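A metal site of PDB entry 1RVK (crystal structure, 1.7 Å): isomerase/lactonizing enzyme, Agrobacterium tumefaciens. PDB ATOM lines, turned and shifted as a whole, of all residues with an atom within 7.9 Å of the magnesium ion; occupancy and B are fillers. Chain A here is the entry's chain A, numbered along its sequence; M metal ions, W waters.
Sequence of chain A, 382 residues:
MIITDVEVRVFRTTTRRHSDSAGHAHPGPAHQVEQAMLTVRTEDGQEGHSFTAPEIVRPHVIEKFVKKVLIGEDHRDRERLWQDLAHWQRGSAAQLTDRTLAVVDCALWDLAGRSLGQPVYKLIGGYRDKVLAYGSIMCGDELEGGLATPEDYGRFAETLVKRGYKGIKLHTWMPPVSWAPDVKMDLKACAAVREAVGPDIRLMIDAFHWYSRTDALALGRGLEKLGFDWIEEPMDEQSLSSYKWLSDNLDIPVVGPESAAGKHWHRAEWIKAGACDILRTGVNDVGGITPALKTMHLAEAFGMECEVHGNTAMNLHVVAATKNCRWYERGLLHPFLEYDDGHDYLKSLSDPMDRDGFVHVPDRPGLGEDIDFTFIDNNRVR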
ATOM      1  N   TYR A 134      10.444 -31.749   4.023  1.00  0.00           N
ATOM      2  CA  TYR A 134       9.536 -30.652   3.751  1.00  0.00           C
ATOM      3  C   TYR A 134       8.678 -31.097   2.579  1.00  0.00           C
ATOM      4  O   TYR A 134       9.132 -31.875   1.734  1.00  0.00           O
ATOM      5  CB  TYR A 134      10.274 -29.331   3.452  1.00  0.00           C
ATOM      6  CG  TYR A 134      11.175 -29.269   2.222  1.00  0.00           C
ATOM      7  CD1 TYR A 134      10.650 -29.113   0.937  1.00  0.00           C
ATOM      8  CD2 TYR A 134      12.562 -29.282   2.369  1.00  0.00           C
ATOM      9  CE1 TYR A 134      11.501 -28.965  -0.176  1.00  0.00           C
ATOM     10  CE2 TYR A 134      13.407 -29.141   1.270  1.00  0.00           C
ATOM     11  CZ  TYR A 134      12.872 -28.980   0.011  1.00  0.00           C
ATOM     12  OH  TYR A 134      13.739 -28.808  -1.055  1.00  0.00           O
ATOM     13  N   SER A 136       7.391 -30.596  -0.773  1.00  0.00           N
ATOM     14  CA  SER A 136       7.747 -29.799  -1.941  1.00  0.00           C
ATOM     15  C   SER A 136       6.586 -29.805  -2.928  1.00  0.00           C
ATOM     16  O   SER A 136       6.327 -30.806  -3.590  1.00  0.00           O
ATOM     17  CB  SER A 136       9.010 -30.394  -2.581  1.00  0.00           C
ATOM     18  OG  SER A 136       9.740 -29.425  -3.311  1.00  0.00           O
ATOM     19  N   LYS A 169       7.659 -26.131   0.830  1.00  0.00           N
ATOM     20  CA  LYS A 169       8.283 -25.305  -0.209  1.00  0.00           C
ATOM     21  C   LYS A 169       7.342 -25.151  -1.392  1.00  0.00           C
ATOM     22  O   LYS A 169       6.807 -26.124  -1.907  1.00  0.00           O
ATOM     23  CB  LYS A 169       9.602 -25.901  -0.699  1.00  0.00           C
ATOM     24  CG  LYS A 169      10.352 -24.954  -1.646  1.00  0.00           C
ATOM     25  CD  LYS A 169      11.756 -25.446  -2.003  1.00  0.00           C
ATOM     26  CE  LYS A 169      11.724 -26.550  -3.051  1.00  0.00           C
ATOM     27  NZ  LYS A 169      13.100 -27.094  -3.294  1.00  0.00           N
ATOM     28  N   LEU A 170       7.137 -23.908  -1.827  1.00  0.00           N
ATOM     29  CA  LEU A 170       6.277 -23.673  -2.974  1.00  0.00           C
ATOM     30  C   LEU A 170       7.091 -23.528  -4.245  1.00  0.00           C
ATOM     31  O   LEU A 170       8.151 -22.914  -4.242  1.00  0.00           O
ATOM     32  CB  LEU A 170       5.478 -22.375  -2.809  1.00  0.00           C
ATOM     33  CG  LEU A 170       4.542 -22.090  -1.645  1.00  0.00           C
ATOM     34  CD1 LEU A 170       3.794 -20.793  -1.966  1.00  0.00           C
ATOM     35  CD2 LEU A 170       3.542 -23.223  -1.455  1.00  0.00           C
ATOM     36  N   HIS A 171       6.596 -24.130  -5.324  1.00  0.00           N
ATOM     37  CA  HIS A 171       7.195 -23.951  -6.641  1.00  0.00           C
ATOM     38  C   HIS A 171       6.022 -23.174  -7.228  1.00  0.00           C
ATOM     39  O   HIS A 171       4.895 -23.687  -7.261  1.00  0.00           O
ATOM     40  CB  HIS A 171       7.357 -25.271  -7.416  1.00  0.00           C
ATOM     41  CG  HIS A 171       8.558 -26.067  -7.006  1.00  0.00           C
ATOM     42  ND1 HIS A 171       8.536 -26.960  -5.942  1.00  0.00           N
ATOM     43  CD2 HIS A 171       9.812 -26.119  -7.512  1.00  0.00           C
ATOM     44  CE1 HIS A 171       9.730 -27.525  -5.825  1.00  0.00           C
ATOM     45  NE2 HIS A 171      10.520 -27.035  -6.760  1.00  0.00           N
ATOM     46  N   MET A 174       4.992 -20.976 -13.714  1.00  0.00           N
ATOM     47  CA  MET A 174       6.008 -20.807 -14.749  1.00  0.00           C
ATOM     48  C   MET A 174       5.434 -21.146 -16.122  1.00  0.00           C
ATOM     49  O   MET A 174       4.522 -21.956 -16.240  1.00  0.00           O
ATOM     50  CB  MET A 174       7.191 -21.737 -14.456  1.00  0.00           C
ATOM     51  CG  MET A 174       7.785 -21.584 -13.062  1.00  0.00           C
ATOM     52  SD  MET A 174       9.286 -22.769 -12.772  1.00  0.00           S
ATOM     53  CE  MET A 174       9.248 -22.819 -10.848  1.00  0.00           C
ATOM     54  N   ILE A 205      10.506 -20.871  -1.020  1.00  0.00           N
ATOM     55  CA  ILE A 205       9.981 -20.651  -2.364  1.00  0.00           C
ATOM     56  C   ILE A 205      11.024 -20.892  -3.437  1.00  0.00           C
ATOM     57  O   ILE A 205      12.159 -20.424  -3.339  1.00  0.00           O
ATOM     58  CB  ILE A 205       9.420 -19.201  -2.502  1.00  0.00           C
ATOM     59  CG1 ILE A 205       9.041 -18.910  -3.960  1.00  0.00           C
ATOM     60  CG2 ILE A 205      10.459 -18.195  -2.033  1.00  0.00           C
ATOM     61  CD1 ILE A 205       7.799 -19.621  -4.416  1.00  0.00           C
ATOM     62  N   ASP A 206      10.604 -21.623  -4.455  1.00  0.00           N
ATOM     63  CA  ASP A 206      11.441 -21.951  -5.617  1.00  0.00           C
ATOM     64  C   ASP A 206      10.595 -21.443  -6.782  1.00  0.00           C
ATOM     65  O   ASP A 206       9.791 -22.177  -7.349  1.00  0.00           O
ATOM     66  CB  ASP A 206      11.633 -23.462  -5.692  1.00  0.00           C
ATOM     67  CG  ASP A 206      12.610 -23.876  -6.770  1.00  0.00           C
ATOM     68  OD1 ASP A 206      12.848 -25.094  -6.879  1.00  0.00           O
ATOM     69  OD2 ASP A 206      13.137 -23.025  -7.512  1.00  0.00           O
ATOM     70  N   ALA A 207      10.777 -20.167  -7.121  1.00  0.00           N
ATOM     71  CA  ALA A 207      10.006 -19.537  -8.183  1.00  0.00           C
ATOM     72  C   ALA A 207      10.631 -19.689  -9.564  1.00  0.00           C
ATOM     73  O   ALA A 207      11.639 -20.359  -9.731  1.00  0.00           O
ATOM     74  CB  ALA A 207       9.827 -18.057  -7.860  1.00  0.00           C
ATOM     75  N   HIS A 209      12.646 -19.949 -12.545  1.00  0.00           N
ATOM     76  CA  HIS A 209      14.104 -20.016 -12.561  1.00  0.00           C
ATOM     77  C   HIS A 209      14.895 -19.046 -13.429  1.00  0.00           C
ATOM     78  O   HIS A 209      16.117 -19.149 -13.501  1.00  0.00           O
ATOM     79  CB  HIS A 209      14.548 -21.432 -12.954  1.00  0.00           C
ATOM     80  CG  HIS A 209      13.756 -22.525 -12.321  1.00  0.00           C
ATOM     81  ND1 HIS A 209      13.701 -22.727 -10.955  1.00  0.00           N
ATOM     82  CD2 HIS A 209      12.999 -23.503 -12.878  1.00  0.00           C
ATOM     83  CE1 HIS A 209      12.952 -23.785 -10.696  1.00  0.00           C
ATOM     84  NE2 HIS A 209      12.509 -24.272 -11.848  1.00  0.00           N
ATOM     85  N   TRP A 230      14.128 -19.506   2.896  1.00  0.00           N
ATOM     86  CA  TRP A 230      15.038 -19.307   1.787  1.00  0.00           C
ATOM     87  C   TRP A 230      14.331 -19.082   0.460  1.00  0.00           C
ATOM     88  O   TRP A 230      13.148 -19.384   0.312  1.00  0.00           O
ATOM     89  CB  TRP A 230      16.029 -20.492   1.661  1.00  0.00           C
ATOM     90  CG  TRP A 230      15.536 -21.780   0.987  1.00  0.00           C
ATOM     91  CD1 TRP A 230      14.907 -21.903  -0.227  1.00  0.00           C
ATOM     92  CD2 TRP A 230      15.736 -23.119   1.462  1.00  0.00           C
ATOM     93  NE1 TRP A 230      14.727 -23.223  -0.537  1.00  0.00           N
ATOM     94  CE2 TRP A 230      15.218 -24.001   0.484  1.00  0.00           C
ATOM     95  CE3 TRP A 230      16.311 -23.670   2.622  1.00  0.00           C
ATOM     96  CZ2 TRP A 230      15.253 -25.395   0.619  1.00  0.00           C
ATOM     97  CZ3 TRP A 230      16.346 -25.064   2.757  1.00  0.00           C
ATOM     98  CH2 TRP A 230      15.822 -25.905   1.768  1.00  0.00           C
ATOM     99  N   GLU A 232      14.868 -19.907  -3.536  1.00  0.00           N
ATOM    100  CA  GLU A 232      15.618 -20.850  -4.355  1.00  0.00           C
ATOM    101  C   GLU A 232      15.576 -20.598  -5.866  1.00  0.00           C
ATOM    102  O   GLU A 232      14.510 -20.445  -6.452  1.00  0.00           O
ATOM    103  CB  GLU A 232      15.084 -22.250  -4.058  1.00  0.00           C
ATOM    104  CG  GLU A 232      15.799 -23.405  -4.741  1.00  0.00           C
ATOM    105  CD  GLU A 232      15.220 -24.738  -4.305  1.00  0.00           C
ATOM    106  OE1 GLU A 232      14.782 -24.844  -3.142  1.00  0.00           O
ATOM    107  OE2 GLU A 232      15.203 -25.670  -5.114  1.00  0.00           O
ATOM    108  N   GLU A 233      16.765 -20.558  -6.468  1.00  0.00           N
ATOM    109  CA  GLU A 233      16.940 -20.369  -7.911  1.00  0.00           C
ATOM    110  C   GLU A 233      15.944 -19.409  -8.577  1.00  0.00           C
ATOM    111  O   GLU A 233      15.170 -19.808  -9.437  1.00  0.00           O
ATOM    112  CB  GLU A 233      16.869 -21.747  -8.598  1.00  0.00           C
ATOM    113  CG  GLU A 233      17.313 -21.763 -10.055  1.00  0.00           C
ATOM    114  CD  GLU A 233      17.476 -23.170 -10.628  1.00  0.00           C
ATOM    115  OE1 GLU A 233      17.914 -23.290 -11.792  1.00  0.00           O
ATOM    116  OE2 GLU A 233      17.172 -24.159  -9.916  1.00  0.00           O
ATOM    117  N   GLU A 237      20.856 -19.613 -13.141  1.00  0.00           N
ATOM    118  CA  GLU A 237      22.054 -20.007 -12.406  1.00  0.00           C
ATOM    119  C   GLU A 237      23.355 -19.970 -13.181  1.00  0.00           C
ATOM    120  O   GLU A 237      24.431 -20.178 -12.619  1.00  0.00           O
ATOM    121  CB  GLU A 237      21.859 -21.374 -11.771  1.00  0.00           C
ATOM    122  CG  GLU A 237      20.934 -21.343 -10.567  1.00  0.00           C
ATOM    123  CD  GLU A 237      20.828 -22.680  -9.875  1.00  0.00           C
ATOM    124  OE1 GLU A 237      20.227 -22.733  -8.782  1.00  0.00           O
ATOM    125  OE2 GLU A 237      21.337 -23.676 -10.427  1.00  0.00           O
ATOM    126  N   VAL A 255      19.604 -19.989  -1.585  1.00  0.00           N
ATOM    127  CA  VAL A 255      20.143 -21.338  -1.650  1.00  0.00           C
ATOM    128  C   VAL A 255      20.412 -21.720  -3.100  1.00  0.00           C
ATOM    129  O   VAL A 255      19.582 -21.445  -3.976  1.00  0.00           O
ATOM    130  CB  VAL A 255      19.175 -22.381  -1.039  1.00  0.00           C
ATOM    131  CG1 VAL A 255      19.806 -23.762  -1.057  1.00  0.00           C
ATOM    132  CG2 VAL A 255      18.825 -21.979   0.369  1.00  0.00           C
ATOM    133  N   GLU A 258      21.233 -25.191  -7.877  1.00  0.00           N
ATOM    134  CA  GLU A 258      20.633 -26.507  -8.050  1.00  0.00           C
ATOM    135  C   GLU A 258      20.929 -27.138  -9.401  1.00  0.00           C
ATOM    136  O   GLU A 258      21.420 -28.254  -9.477  1.00  0.00           O
ATOM    137  CB  GLU A 258      19.113 -26.460  -7.884  1.00  0.00           C
ATOM    138  CG  GLU A 258      18.482 -27.836  -8.017  1.00  0.00           C
ATOM    139  CD  GLU A 258      16.978 -27.805  -8.034  1.00  0.00           C
ATOM    140  OE1 GLU A 258      16.388 -27.323  -7.058  1.00  0.00           O
ATOM    141  OE2 GLU A 258      16.387 -28.266  -9.030  1.00  0.00           O
ATOM    142  N   SER A 259      20.629 -26.402 -10.475  1.00  0.00           N
ATOM    143  CA  SER A 259      20.805 -26.918 -11.831  1.00  0.00           C
ATOM    144  C   SER A 259      22.130 -26.650 -12.528  1.00  0.00           C
ATOM    145  O   SER A 259      22.439 -27.307 -13.510  1.00  0.00           O
ATOM    146  CB  SER A 259      19.660 -26.401 -12.717  1.00  0.00           C
ATOM    147  OG  SER A 259      19.705 -24.992 -12.856  1.00  0.00           O
ATOM    148  N   ARG A 280      23.582 -25.942  -2.491  1.00  0.00           N
ATOM    149  CA  ARG A 280      22.614 -26.928  -2.939  1.00  0.00           C
ATOM    150  C   ARG A 280      23.321 -27.952  -3.811  1.00  0.00           C
ATOM    151  O   ARG A 280      24.290 -27.637  -4.501  1.00  0.00           O
ATOM    152  CB  ARG A 280      21.481 -26.266  -3.726  1.00  0.00           C
ATOM    153  CG  ARG A 280      20.287 -27.201  -4.029  1.00  0.00           C
ATOM    154  CD  ARG A 280      19.016 -26.358  -4.167  1.00  0.00           C
ATOM    155  NE  ARG A 280      17.786 -27.091  -4.462  1.00  0.00           N
ATOM    156  CZ  ARG A 280      17.170 -27.936  -3.646  1.00  0.00           C
ATOM    157  NH1 ARG A 280      16.037 -28.524  -4.025  1.00  0.00           N
ATOM    158  NH2 ARG A 280      17.681 -28.224  -2.447  1.00  0.00           N
ATOM    159  N   ASP A 285      21.924 -33.858 -10.061  1.00  0.00           N
ATOM    160  CA  ASP A 285      22.541 -32.611 -10.466  1.00  0.00           C
ATOM    161  C   ASP A 285      24.060 -32.604 -10.535  1.00  0.00           C
ATOM    162  O   ASP A 285      24.631 -31.884 -11.358  1.00  0.00           O
ATOM    163  CB  ASP A 285      22.072 -31.491  -9.542  1.00  0.00           C
ATOM    164  CG  ASP A 285      20.558 -31.369  -9.503  1.00  0.00           C
ATOM    165  OD1 ASP A 285      19.955 -31.044 -10.552  1.00  0.00           O
ATOM    166  OD2 ASP A 285      19.982 -31.613  -8.424  1.00  0.00           O
ATOM    167  N   HIS A 309      18.697 -31.651  -3.375  1.00  0.00           N
ATOM    168  CA  HIS A 309      17.571 -31.573  -4.304  1.00  0.00           C
ATOM    169  C   HIS A 309      17.087 -32.928  -4.771  1.00  0.00           C
ATOM    170  O   HIS A 309      17.880 -33.741  -5.240  1.00  0.00           O
ATOM    171  CB  HIS A 309      17.949 -30.747  -5.539  1.00  0.00           C
ATOM    172  CG  HIS A 309      16.978 -30.899  -6.673  1.00  0.00           C
ATOM    173  ND1 HIS A 309      17.364 -31.359  -7.919  1.00  0.00           N
ATOM    174  CD2 HIS A 309      15.643 -30.681  -6.742  1.00  0.00           C
ATOM    175  CE1 HIS A 309      16.302 -31.418  -8.706  1.00  0.00           C
ATOM    176  NE2 HIS A 309      15.248 -31.010  -8.022  1.00  0.00           N
ATOM    177  N   GLY A 310      15.781 -33.153  -4.657  1.00  0.00           N
ATOM    178  CA  GLY A 310      15.207 -34.391  -5.142  1.00  0.00           C
ATOM    179  C   GLY A 310      14.860 -35.456  -4.131  1.00  0.00           C
ATOM    180  O   GLY A 310      15.515 -35.596  -3.093  1.00  0.00           O
ATOM    181  N   GLU A 329      13.930 -33.652   0.683  1.00  0.00           N
ATOM    182  CA  GLU A 329      12.873 -33.048  -0.126  1.00  0.00           C
ATOM    183  C   GLU A 329      11.880 -34.119  -0.558  1.00  0.00           C
ATOM    184  O   GLU A 329      12.205 -34.973  -1.373  1.00  0.00           O
ATOM    185  CB  GLU A 329      13.489 -32.368  -1.352  1.00  0.00           C
ATOM    186  CG  GLU A 329      12.468 -31.633  -2.205  1.00  0.00           C
ATOM    187  CD  GLU A 329      13.105 -30.762  -3.263  1.00  0.00           C
ATOM    188  OE1 GLU A 329      12.352 -30.055  -3.952  1.00  0.00           O
ATOM    189  OE2 GLU A 329      14.355 -30.788  -3.416  1.00  0.00           O
ATOM    190  N   LEU A 332       7.625 -34.222  -5.924  1.00  0.00           N
ATOM    191  CA  LEU A 332       6.696 -33.101  -5.802  1.00  0.00           C
ATOM    192  C   LEU A 332       5.271 -33.518  -5.450  1.00  0.00           C
ATOM    193  O   LEU A 332       4.800 -34.580  -5.847  1.00  0.00           O
ATOM    194  CB  LEU A 332       6.701 -32.297  -7.107  1.00  0.00           C
ATOM    195  CG  LEU A 332       8.077 -31.727  -7.455  1.00  0.00           C
ATOM    196  CD1 LEU A 332       8.013 -30.985  -8.780  1.00  0.00           C
ATOM    197  CD2 LEU A 332       8.547 -30.800  -6.358  1.00  0.00           C
HETATM  198 MG    MG M   1      14.557 -26.300  -7.091  1.00  0.00          MG
HETATM  199  O   HOH W   1      13.949 -27.304  -9.057  1.00  0.00           O
HETATM  200  O   HOH W   2      13.254 -27.885  -6.081  1.00  0.00           O
HETATM  201  O   HOH W   3      15.422 -24.553  -8.194  1.00  0.00           O
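The side-chain carboxylate (OE1) of Glu 258 lies close to the guanidinium group (NE) of Arg 280. NE2 of His 309 lies within hydrogen-bond range of OE2 of Glu 258 (3.1 Å). A ring nitrogen (NE2) of His 171 sits close to the side-chain carboxylate of Asp 206, 3.0 Å away. N of Asp 206 is in hydrogen-bond range of O of Leu 170, 2.8 Å away. The side-chain carboxylate (OE1) of Glu 232 lies within salt-bridge range of the guanidinium group (NE) of Arg 280, at 3.98 Å. NZ of Lys 169 is in salt-bridge range of OE1 of Glu 232 (2.8 Å). The side-chain carboxylate of Glu 232 is in hydrogen-bond range of the indole nitrogen of Trp 230 (3.1 Å). N of Glu 232 lies within hydrogen-bond range of O of Ile 205.
Three residues have an atom within 4 Å of the magnesium ion: Asp 206, Glu 232 and Glu 258.
The magnesium ion is bound by OE1 of Glu 258 (2.1 Å). The side-chain carboxylate (OD1) of Asp 206 is bound to the magnesium ion. The magnesium ion is bound by OE2 of Glu 232 (2.2 Å). Water W3 binds the magnesium ion (2.2 Å). The magnesium ion is bound by water W2 (2.3 Å). Water W1 binds the magnesium ion (2.3 Å).
Water W3 lies within hydrogen-bond range of OE2 of Glu 233 (2.5 Å) and OD2 of Asp 206 (2.8 Å). Water W2 lies within hydrogen-bond range of the side-chain amino group of Lys 169 (2.9 Å), a ring nitrogen (NE2) of His 171 (2.9 Å) and the side-chain carboxylate of Glu 329 (3.2 Å).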
